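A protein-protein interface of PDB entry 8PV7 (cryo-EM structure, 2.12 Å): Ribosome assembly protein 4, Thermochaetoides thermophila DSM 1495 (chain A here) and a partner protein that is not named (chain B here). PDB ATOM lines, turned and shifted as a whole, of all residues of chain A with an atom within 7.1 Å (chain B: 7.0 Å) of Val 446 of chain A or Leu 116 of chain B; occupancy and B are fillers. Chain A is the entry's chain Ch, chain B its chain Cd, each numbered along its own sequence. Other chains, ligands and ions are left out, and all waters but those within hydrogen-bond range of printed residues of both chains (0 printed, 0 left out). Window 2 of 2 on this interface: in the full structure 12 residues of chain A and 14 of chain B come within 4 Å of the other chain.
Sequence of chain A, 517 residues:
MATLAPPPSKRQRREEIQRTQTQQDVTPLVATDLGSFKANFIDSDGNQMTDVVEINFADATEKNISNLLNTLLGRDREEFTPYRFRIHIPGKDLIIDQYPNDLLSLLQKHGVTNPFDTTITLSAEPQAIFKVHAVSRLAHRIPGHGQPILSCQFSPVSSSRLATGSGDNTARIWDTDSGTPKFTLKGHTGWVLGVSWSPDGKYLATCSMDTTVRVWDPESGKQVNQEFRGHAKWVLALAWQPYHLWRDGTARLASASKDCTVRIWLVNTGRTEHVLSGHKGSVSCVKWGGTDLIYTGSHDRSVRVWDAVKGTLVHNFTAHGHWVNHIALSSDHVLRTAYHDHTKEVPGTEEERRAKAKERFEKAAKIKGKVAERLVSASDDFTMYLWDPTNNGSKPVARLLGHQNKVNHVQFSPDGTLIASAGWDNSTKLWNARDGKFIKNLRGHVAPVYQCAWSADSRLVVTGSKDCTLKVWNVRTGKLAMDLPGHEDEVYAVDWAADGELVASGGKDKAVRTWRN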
ATOM      1  N   ASP A 425     -20.893  27.215  -9.314  1.00  0.00           N
ATOM      2  CA  ASP A 425     -22.245  26.736  -9.076  1.00  0.00           C
ATOM      3  C   ASP A 425     -22.281  25.654  -8.004  1.00  0.00           C
ATOM      4  O   ASP A 425     -23.171  24.799  -8.023  1.00  0.00           O
ATOM      5  CB  ASP A 425     -22.861  26.220 -10.378  1.00  0.00           C
ATOM      6  CG  ASP A 425     -21.992  25.187 -11.070  1.00  0.00           C
ATOM      7  OD1 ASP A 425     -20.838  24.982 -10.647  1.00  0.00           O
ATOM      8  OD2 ASP A 425     -22.461  24.572 -12.042  1.00  0.00           O
ATOM      9  N   ASN A 426     -21.315  25.679  -7.081  1.00  0.00           N
ATOM     10  CA  ASN A 426     -21.161  24.755  -5.961  1.00  0.00           C
ATOM     11  C   ASN A 426     -21.013  23.306  -6.395  1.00  0.00           C
ATOM     12  O   ASN A 426     -21.408  22.404  -5.658  1.00  0.00           O
ATOM     13  CB  ASN A 426     -22.321  24.859  -4.960  1.00  0.00           C
ATOM     14  CG  ASN A 426     -22.859  26.259  -4.826  1.00  0.00           C
ATOM     15  OD1 ASN A 426     -22.181  27.231  -5.142  1.00  0.00           O
ATOM     16  ND2 ASN A 426     -24.095  26.370  -4.372  1.00  0.00           N
ATOM     17  N   SER A 427     -20.451  23.037  -7.567  1.00  0.00           N
ATOM     18  CA  SER A 427     -20.394  21.672  -8.062  1.00  0.00           C
ATOM     19  C   SER A 427     -19.040  21.368  -8.685  1.00  0.00           C
ATOM     20  O   SER A 427     -18.360  22.238  -9.235  1.00  0.00           O
ATOM     21  CB  SER A 427     -21.510  21.393  -9.078  1.00  0.00           C
ATOM     22  OG  SER A 427     -21.215  21.965 -10.335  1.00  0.00           O
ATOM     23  N   ARG A 443     -22.103  16.559  -6.035  1.00  0.00           N
ATOM     24  CA  ARG A 443     -22.976  17.583  -5.476  1.00  0.00           C
ATOM     25  C   ARG A 443     -22.984  17.461  -3.950  1.00  0.00           C
ATOM     26  O   ARG A 443     -23.763  16.702  -3.372  1.00  0.00           O
ATOM     27  CB  ARG A 443     -24.383  17.460  -6.063  1.00  0.00           C
ATOM     28  CG  ARG A 443     -25.325  18.585  -5.700  1.00  0.00           C
ATOM     29  CD  ARG A 443     -26.751  18.231  -6.064  1.00  0.00           C
ATOM     30  NE  ARG A 443     -27.697  19.262  -5.659  1.00  0.00           N
ATOM     31  CZ  ARG A 443     -29.000  19.214  -5.895  1.00  0.00           C
ATOM     32  NH1 ARG A 443     -29.551  18.189  -6.522  1.00  0.00           N
ATOM     33  NH2 ARG A 443     -29.768  20.226  -5.505  1.00  0.00           N
ATOM     34  N   GLY A 444     -22.083  18.186  -3.296  1.00  0.00           N
ATOM     35  CA  GLY A 444     -22.140  18.288  -1.853  1.00  0.00           C
ATOM     36  C   GLY A 444     -21.836  19.655  -1.279  1.00  0.00           C
ATOM     37  O   GLY A 444     -22.168  19.929  -0.124  1.00  0.00           O
ATOM     38  N   HIS A 445     -21.232  20.535  -2.065  1.00  0.00           N
ATOM     39  CA  HIS A 445     -20.799  21.833  -1.569  1.00  0.00           C
ATOM     40  C   HIS A 445     -21.956  22.815  -1.659  1.00  0.00           C
ATOM     41  O   HIS A 445     -22.834  22.666  -2.512  1.00  0.00           O
ATOM     42  CB  HIS A 445     -19.601  22.357  -2.357  1.00  0.00           C
ATOM     43  CG  HIS A 445     -18.297  21.759  -1.939  1.00  0.00           C
ATOM     44  ND1 HIS A 445     -17.767  21.936  -0.681  1.00  0.00           N
ATOM     45  CD2 HIS A 445     -17.397  21.016  -2.624  1.00  0.00           C
ATOM     46  CE1 HIS A 445     -16.605  21.315  -0.604  1.00  0.00           C
ATOM     47  NE2 HIS A 445     -16.356  20.751  -1.770  1.00  0.00           N
ATOM     48  N   VAL A 446     -21.952  23.818  -0.783  1.00  0.00           N
ATOM     49  CA  VAL A 446     -23.069  24.756  -0.738  1.00  0.00           C
ATOM     50  C   VAL A 446     -22.620  26.142  -1.179  1.00  0.00           C
ATOM     51  O   VAL A 446     -23.437  27.053  -1.344  1.00  0.00           O
ATOM     52  CB  VAL A 446     -23.690  24.775   0.671  1.00  0.00           C
ATOM     53  CG1 VAL A 446     -24.617  23.591   0.853  1.00  0.00           C
ATOM     54  CG2 VAL A 446     -22.616  24.781   1.732  1.00  0.00           C
ATOM     55  N   ALA A 447     -21.324  26.326  -1.355  1.00  0.00           N
ATOM     56  CA  ALA A 447     -20.704  27.546  -1.838  1.00  0.00           C
ATOM     57  C   ALA A 447     -19.836  27.223  -3.049  1.00  0.00           C
ATOM     58  O   ALA A 447     -19.631  26.050  -3.375  1.00  0.00           O
ATOM     59  CB  ALA A 447     -19.870  28.186  -0.718  1.00  0.00           C
ATOM     60  N   PRO A 448     -19.340  28.259  -3.789  1.00  0.00           N
ATOM     61  CA  PRO A 448     -18.409  27.993  -4.896  1.00  0.00           C
ATOM     62  C   PRO A 448     -17.193  27.156  -4.537  1.00  0.00           C
ATOM     63  O   PRO A 448     -16.599  27.307  -3.468  1.00  0.00           O
ATOM     64  CB  PRO A 448     -17.985  29.402  -5.321  1.00  0.00           C
ATOM     65  CG  PRO A 448     -19.167  30.209  -5.079  1.00  0.00           C
ATOM     66  CD  PRO A 448     -19.884  29.627  -3.896  1.00  0.00           C
ATOM     67  N   VAL A 449     -16.838  26.248  -5.431  1.00  0.00           N
ATOM     68  CA  VAL A 449     -15.718  25.341  -5.237  1.00  0.00           C
ATOM     69  C   VAL A 449     -14.513  25.963  -5.916  1.00  0.00           C
ATOM     70  O   VAL A 449     -14.545  26.235  -7.120  1.00  0.00           O
ATOM     71  CB  VAL A 449     -16.026  23.948  -5.805  1.00  0.00           C
ATOM     72  CG1 VAL A 449     -14.959  22.959  -5.388  1.00  0.00           C
ATOM     73  CG2 VAL A 449     -17.390  23.494  -5.343  1.00  0.00           C
ATOM     74  N   SER A 465     -13.551  24.358  -0.930  1.00  0.00           N
ATOM     75  CA  SER A 465     -14.583  25.309  -1.314  1.00  0.00           C
ATOM     76  C   SER A 465     -14.604  26.546  -0.425  1.00  0.00           C
ATOM     77  O   SER A 465     -13.895  26.652   0.575  1.00  0.00           O
ATOM     78  CB  SER A 465     -15.960  24.643  -1.298  1.00  0.00           C
ATOM     79  OG  SER A 465     -16.996  25.591  -1.427  1.00  0.00           O
ATOM     80  N   LYS A 466     -15.453  27.487  -0.830  1.00  0.00           N
ATOM     81  CA  LYS A 466     -15.729  28.706  -0.085  1.00  0.00           C
ATOM     82  C   LYS A 466     -16.581  28.443   1.152  1.00  0.00           C
ATOM     83  O   LYS A 466     -16.567  29.255   2.082  1.00  0.00           O
ATOM     84  CB  LYS A 466     -16.398  29.713  -1.033  1.00  0.00           C
ATOM     85  CG  LYS A 466     -16.745  31.066  -0.446  1.00  0.00           C
ATOM     86  CD  LYS A 466     -17.473  31.935  -1.440  1.00  0.00           C
ATOM     87  CE  LYS A 466     -17.810  33.277  -0.833  1.00  0.00           C
ATOM     88  NZ  LYS A 466     -18.662  34.090  -1.728  1.00  0.00           N
ATOM     89  N   ASP A 467     -17.260  27.296   1.227  1.00  0.00           N
ATOM     90  CA  ASP A 467     -18.066  26.957   2.394  1.00  0.00           C
ATOM     91  C   ASP A 467     -17.236  26.437   3.564  1.00  0.00           C
ATOM     92  O   ASP A 467     -17.811  25.857   4.489  1.00  0.00           O
ATOM     93  CB  ASP A 467     -19.157  25.936   2.028  1.00  0.00           C
ATOM     94  CG  ASP A 467     -18.612  24.580   1.565  1.00  0.00           C
ATOM     95  OD1 ASP A 467     -17.391  24.350   1.522  1.00  0.00           O
ATOM     96  OD2 ASP A 467     -19.441  23.719   1.217  1.00  0.00           O
ATOM     97  N   THR A 469     -14.991  23.993   3.738  1.00  0.00           N
ATOM     98  CA  THR A 469     -14.792  22.557   3.866  1.00  0.00           C
ATOM     99  C   THR A 469     -14.004  21.990   2.689  1.00  0.00           C
ATOM    100  O   THR A 469     -13.943  22.574   1.589  1.00  0.00           O
ATOM    101  CB  THR A 469     -16.124  21.789   3.976  1.00  0.00           C
ATOM    102  OG1 THR A 469     -16.750  21.712   2.691  1.00  0.00           O
ATOM    103  CG2 THR A 469     -17.073  22.440   4.964  1.00  0.00           C
ATOM    104  N   LYS A 471     -13.916  18.242   0.579  1.00  0.00           N
ATOM    105  CA  LYS A 471     -14.667  17.015   0.370  1.00  0.00           C
ATOM    106  C   LYS A 471     -13.877  16.083  -0.527  1.00  0.00           C
ATOM    107  O   LYS A 471     -13.391  16.489  -1.582  1.00  0.00           O
ATOM    108  CB  LYS A 471     -16.049  17.288  -0.225  1.00  0.00           C
ATOM    109  CG  LYS A 471     -16.949  18.085   0.687  1.00  0.00           C
ATOM    110  CD  LYS A 471     -18.381  18.072   0.241  1.00  0.00           C
ATOM    111  CE  LYS A 471     -19.168  19.132   0.970  1.00  0.00           C
ATOM    112  NZ  LYS A 471     -18.935  19.103   2.433  1.00  0.00           N
ATOM    113  N   ILE B  83     -29.010  20.109   8.702  1.00  0.00           N
ATOM    114  CA  ILE B  83     -29.245  18.889   7.940  1.00  0.00           C
ATOM    115  C   ILE B  83     -27.900  18.281   7.568  1.00  0.00           C
ATOM    116  O   ILE B  83     -26.933  18.998   7.294  1.00  0.00           O
ATOM    117  CB  ILE B  83     -30.137  19.153   6.699  1.00  0.00           C
ATOM    118  CG1 ILE B  83     -30.589  17.843   6.053  1.00  0.00           C
ATOM    119  CG2 ILE B  83     -29.459  20.064   5.679  1.00  0.00           C
ATOM    120  CD1 ILE B  83     -31.711  18.008   5.065  1.00  0.00           C
ATOM    121  N   GLN B  85     -25.343  15.696   5.262  1.00  0.00           N
ATOM    122  CA  GLN B  85     -25.128  15.408   3.848  1.00  0.00           C
ATOM    123  C   GLN B  85     -25.797  14.101   3.438  1.00  0.00           C
ATOM    124  O   GLN B  85     -26.308  13.983   2.319  1.00  0.00           O
ATOM    125  CB  GLN B  85     -23.629  15.360   3.545  1.00  0.00           C
ATOM    126  CG  GLN B  85     -22.905  16.692   3.672  1.00  0.00           C
ATOM    127  CD  GLN B  85     -23.066  17.579   2.449  1.00  0.00           C
ATOM    128  OE1 GLN B  85     -23.574  17.148   1.419  1.00  0.00           O
ATOM    129  NE2 GLN B  85     -22.631  18.825   2.561  1.00  0.00           N
ATOM    130  N   LEU B  88     -29.428  14.846   3.038  1.00  0.00           N
ATOM    131  CA  LEU B  88     -29.628  15.561   1.781  1.00  0.00           C
ATOM    132  C   LEU B  88     -29.568  14.615   0.587  1.00  0.00           C
ATOM    133  O   LEU B  88     -30.369  14.737  -0.345  1.00  0.00           O
ATOM    134  CB  LEU B  88     -28.593  16.671   1.626  1.00  0.00           C
ATOM    135  CG  LEU B  88     -28.885  17.986   2.341  1.00  0.00           C
ATOM    136  CD1 LEU B  88     -27.672  18.891   2.298  1.00  0.00           C
ATOM    137  CD2 LEU B  88     -30.088  18.664   1.719  1.00  0.00           C
ATOM    138  N   GLN B  89     -28.636  13.661   0.604  1.00  0.00           N
ATOM    139  CA  GLN B  89     -28.523  12.720  -0.507  1.00  0.00           C
ATOM    140  C   GLN B  89     -29.742  11.803  -0.587  1.00  0.00           C
ATOM    141  O   GLN B  89     -30.231  11.500  -1.685  1.00  0.00           O
ATOM    142  CB  GLN B  89     -27.235  11.909  -0.374  1.00  0.00           C
ATOM    143  CG  GLN B  89     -26.990  10.930  -1.505  1.00  0.00           C
ATOM    144  CD  GLN B  89     -26.830  11.616  -2.851  1.00  0.00           C
ATOM    145  OE1 GLN B  89     -26.321  12.734  -2.940  1.00  0.00           O
ATOM    146  NE2 GLN B  89     -27.269  10.946  -3.908  1.00  0.00           N
ATOM    147  N   PHE B  91     -32.750  12.641   0.374  1.00  0.00           N
ATOM    148  CA  PHE B  91     -33.854  13.451  -0.129  1.00  0.00           C
ATOM    149  C   PHE B  91     -33.715  13.731  -1.622  1.00  0.00           C
ATOM    150  O   PHE B  91     -34.719  13.853  -2.329  1.00  0.00           O
ATOM    151  CB  PHE B  91     -33.951  14.751   0.662  1.00  0.00           C
ATOM    152  CG  PHE B  91     -34.655  14.601   1.972  1.00  0.00           C
ATOM    153  CD1 PHE B  91     -35.733  13.744   2.096  1.00  0.00           C
ATOM    154  CD2 PHE B  91     -34.252  15.324   3.078  1.00  0.00           C
ATOM    155  CE1 PHE B  91     -36.390  13.608   3.300  1.00  0.00           C
ATOM    156  CE2 PHE B  91     -34.906  15.190   4.281  1.00  0.00           C
ATOM    157  CZ  PHE B  91     -35.974  14.333   4.394  1.00  0.00           C
ATOM    158  N   ARG B  92     -32.482  13.833  -2.123  1.00  0.00           N
ATOM    159  CA  ARG B  92     -32.283  13.972  -3.566  1.00  0.00           C
ATOM    160  C   ARG B  92     -32.687  12.702  -4.305  1.00  0.00           C
ATOM    161  O   ARG B  92     -33.247  12.764  -5.406  1.00  0.00           O
ATOM    162  CB  ARG B  92     -30.829  14.320  -3.872  1.00  0.00           C
ATOM    163  CG  ARG B  92     -30.411  15.691  -3.403  1.00  0.00           C
ATOM    164  CD  ARG B  92     -29.061  16.072  -3.955  1.00  0.00           C
ATOM    165  NE  ARG B  92     -28.500  17.219  -3.255  1.00  0.00           N
ATOM    166  CZ  ARG B  92     -27.531  17.147  -2.354  1.00  0.00           C
ATOM    167  NH1 ARG B  92     -26.967  15.995  -2.037  1.00  0.00           N
ATOM    168  NH2 ARG B  92     -27.113  18.261  -1.761  1.00  0.00           N
ATOM    169  N   PRO B 113     -35.032  22.311   3.155  1.00  0.00           N
ATOM    170  CA  PRO B 113     -34.284  23.229   2.278  1.00  0.00           C
ATOM    171  C   PRO B 113     -34.316  22.736   0.832  1.00  0.00           C
ATOM    172  O   PRO B 113     -33.409  22.078   0.329  1.00  0.00           O
ATOM    173  CB  PRO B 113     -32.879  23.198   2.880  1.00  0.00           C
ATOM    174  CG  PRO B 113     -32.770  21.857   3.493  1.00  0.00           C
ATOM    175  CD  PRO B 113     -34.135  21.476   3.971  1.00  0.00           C
ATOM    176  N   MET B 114     -35.409  23.068   0.139  1.00  0.00           N
ATOM    177  CA  MET B 114     -35.667  22.492  -1.177  1.00  0.00           C
ATOM    178  C   MET B 114     -34.686  22.976  -2.236  1.00  0.00           C
ATOM    179  O   MET B 114     -34.516  22.312  -3.261  1.00  0.00           O
ATOM    180  CB  MET B 114     -37.099  22.792  -1.614  1.00  0.00           C
ATOM    181  CG  MET B 114     -38.162  22.146  -0.749  1.00  0.00           C
ATOM    182  SD  MET B 114     -37.952  20.363  -0.571  1.00  0.00           S
ATOM    183  CE  MET B 114     -38.063  19.812  -2.268  1.00  0.00           C
ATOM    184  N   SER B 115     -34.023  24.111  -2.013  1.00  0.00           N
ATOM    185  CA  SER B 115     -33.020  24.574  -2.967  1.00  0.00           C
ATOM    186  C   SER B 115     -31.754  23.728  -2.932  1.00  0.00           C
ATOM    187  O   SER B 115     -30.961  23.784  -3.875  1.00  0.00           O
ATOM    188  CB  SER B 115     -32.679  26.042  -2.713  1.00  0.00           C
ATOM    189  OG  SER B 115     -32.034  26.214  -1.466  1.00  0.00           O
ATOM    190  N   LEU B 116     -31.540  22.959  -1.867  1.00  0.00           N
ATOM    191  CA  LEU B 116     -30.437  22.011  -1.785  1.00  0.00           C
ATOM    192  C   LEU B 116     -30.840  20.601  -2.180  1.00  0.00           C
ATOM    193  O   LEU B 116     -29.992  19.707  -2.182  1.00  0.00           O
ATOM    194  CB  LEU B 116     -29.861  21.987  -0.367  1.00  0.00           C
ATOM    195  CG  LEU B 116     -29.491  23.317   0.281  1.00  0.00           C
ATOM    196  CD1 LEU B 116     -29.308  23.121   1.767  1.00  0.00           C
ATOM    197  CD2 LEU B 116     -28.233  23.872  -0.343  1.00  0.00           C
ATOM    198  N   ILE B 117     -32.112  20.380  -2.511  1.00  0.00           N
ATOM    199  CA  ILE B 117     -32.638  19.054  -2.787  1.00  0.00           C
ATOM    200  C   ILE B 117     -33.108  18.917  -4.228  1.00  0.00           C
ATOM    201  O   ILE B 117     -32.836  17.903  -4.879  1.00  0.00           O
ATOM    202  CB  ILE B 117     -33.780  18.703  -1.806  1.00  0.00           C
ATOM    203  CG1 ILE B 117     -33.269  18.750  -0.366  1.00  0.00           C
ATOM    204  CG2 ILE B 117     -34.392  17.346  -2.125  1.00  0.00           C
ATOM    205  CD1 ILE B 117     -34.342  18.612   0.671  1.00  0.00           C
ATOM    206  N   ARG B 118     -33.793  19.930  -4.752  1.00  0.00           N
ATOM    207  CA  ARG B 118     -34.374  19.833  -6.082  1.00  0.00           C
ATOM    208  C   ARG B 118     -33.289  19.847  -7.152  1.00  0.00           C
ATOM    209  O   ARG B 118     -32.179  20.341  -6.940  1.00  0.00           O
ATOM    210  CB  ARG B 118     -35.356  20.979  -6.321  1.00  0.00           C
ATOM    211  CG  ARG B 118     -34.699  22.334  -6.493  1.00  0.00           C
ATOM    212  CD  ARG B 118     -35.699  23.390  -6.914  1.00  0.00           C
ATOM    213  NE  ARG B 118     -36.786  23.537  -5.955  1.00  0.00           N
ATOM    214  CZ  ARG B 118     -36.934  24.579  -5.152  1.00  0.00           C
ATOM    215  NH1 ARG B 118     -36.061  25.572  -5.143  1.00  0.00           N
ATOM    216  NH2 ARG B 118     -37.985  24.629  -4.340  1.00  0.00           N
ATOM    217  N   ASP B 119     -33.615  19.269  -8.304  1.00  0.00           N
ATOM    218  CA  ASP B 119     -32.684  19.232  -9.419  1.00  0.00           C
ATOM    219  C   ASP B 119     -32.477  20.629  -9.992  1.00  0.00           C
ATOM    220  O   ASP B 119     -33.389  21.458 -10.034  1.00  0.00           O
ATOM    221  CB  ASP B 119     -33.190  18.290 -10.509  1.00  0.00           C
ATOM    222  CG  ASP B 119     -33.399  16.880 -10.005  1.00  0.00           C
ATOM    223  OD1 ASP B 119     -34.564  16.431  -9.950  1.00  0.00           O
ATOM    224  OD2 ASP B 119     -32.397  16.220  -9.662  1.00  0.00           O
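The side-chain amide nitrogen (NE2) of Gln 85 of chain B lies within hydrogen-bond range of the backbone carbonyl oxygen (O) of Gly 444 of chain A, at 2.9 Å.
O of Leu 116 of chain B is in hydrogen-bond range of NH2 of Arg 443 of chain A.
The guanidinium group (NH2) of Arg 443 of chain A lies within hydrogen-bond range of the backbone carbonyl oxygen (O) of Arg 118 of chain B.
NE of Arg 443 of chain A lies close to NE of Arg 92 of chain B, at 3.3 Å.
OE1 of Gln 89 of chain B sits at hydrogen-bond distance from NH1 of Arg 92 of chain B (3.4 Å).
The backbone carbonyl oxygen of Leu 116 of chain B is in hydrogen-bond range of the guanidinium group of Arg 92 of chain B, at 3.1 Å.
ND2 of Asn 426 of chain A lies within hydrogen-bond range of O of Val 446 of chain A (3.2 Å).
OD2 of Asp 467 of chain A is in hydrogen-bond range of N of Val 446 of chain A.
The side-chain amino group of Lys 471 of chain A lies within hydrogen-bond range of the side-chain hydroxyl of Thr 469 of chain A (3.4 Å).
Among the printed residues, merely in contact across the chains: Arg 443 of chain A with Ile 117 of chain B (3.7 Å), Lys 471 of chain A with Gln 85 of chain B (3.7 Å) and Val 446 of chain A with Leu 116 of chain B (3.8 Å).
Of the printed residues of chain B, Gly 444 of chain A touches Gln 85 (2.9 Å).
Of the printed residues of chain B, Val 446 of chain A touches Leu 116.
Lys 466 of chain A touches none of the printed residues of chain B.
Of the printed residues of chain A, Gln 85 of chain B touches Gly 444 (2.9 Å) and Lys 471 (3.7 Å).
Of the printed residues of chain A, Arg 92 of chain B touches Arg 443 (3.3 Å).
Of chain A, only Arg 443 and Val 446 come within 4 Å of Leu 116 of chain B.
Printed residues of chain A within 4 Å of Ile 117 of chain B: Arg 443 (3.7 Å).
The nearest residue of chain B that does not touch Val 446 of chain A is Gln 85 of chain B (5.4 Å).
Hydrophobic or aromatic side chains of chain A that line the printed part of chain B: Val 446.
Among the printed residues, no Asp or Glu carboxylate lies within 4 Å of a Lys or Arg side-chain nitrogen of the other chain.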
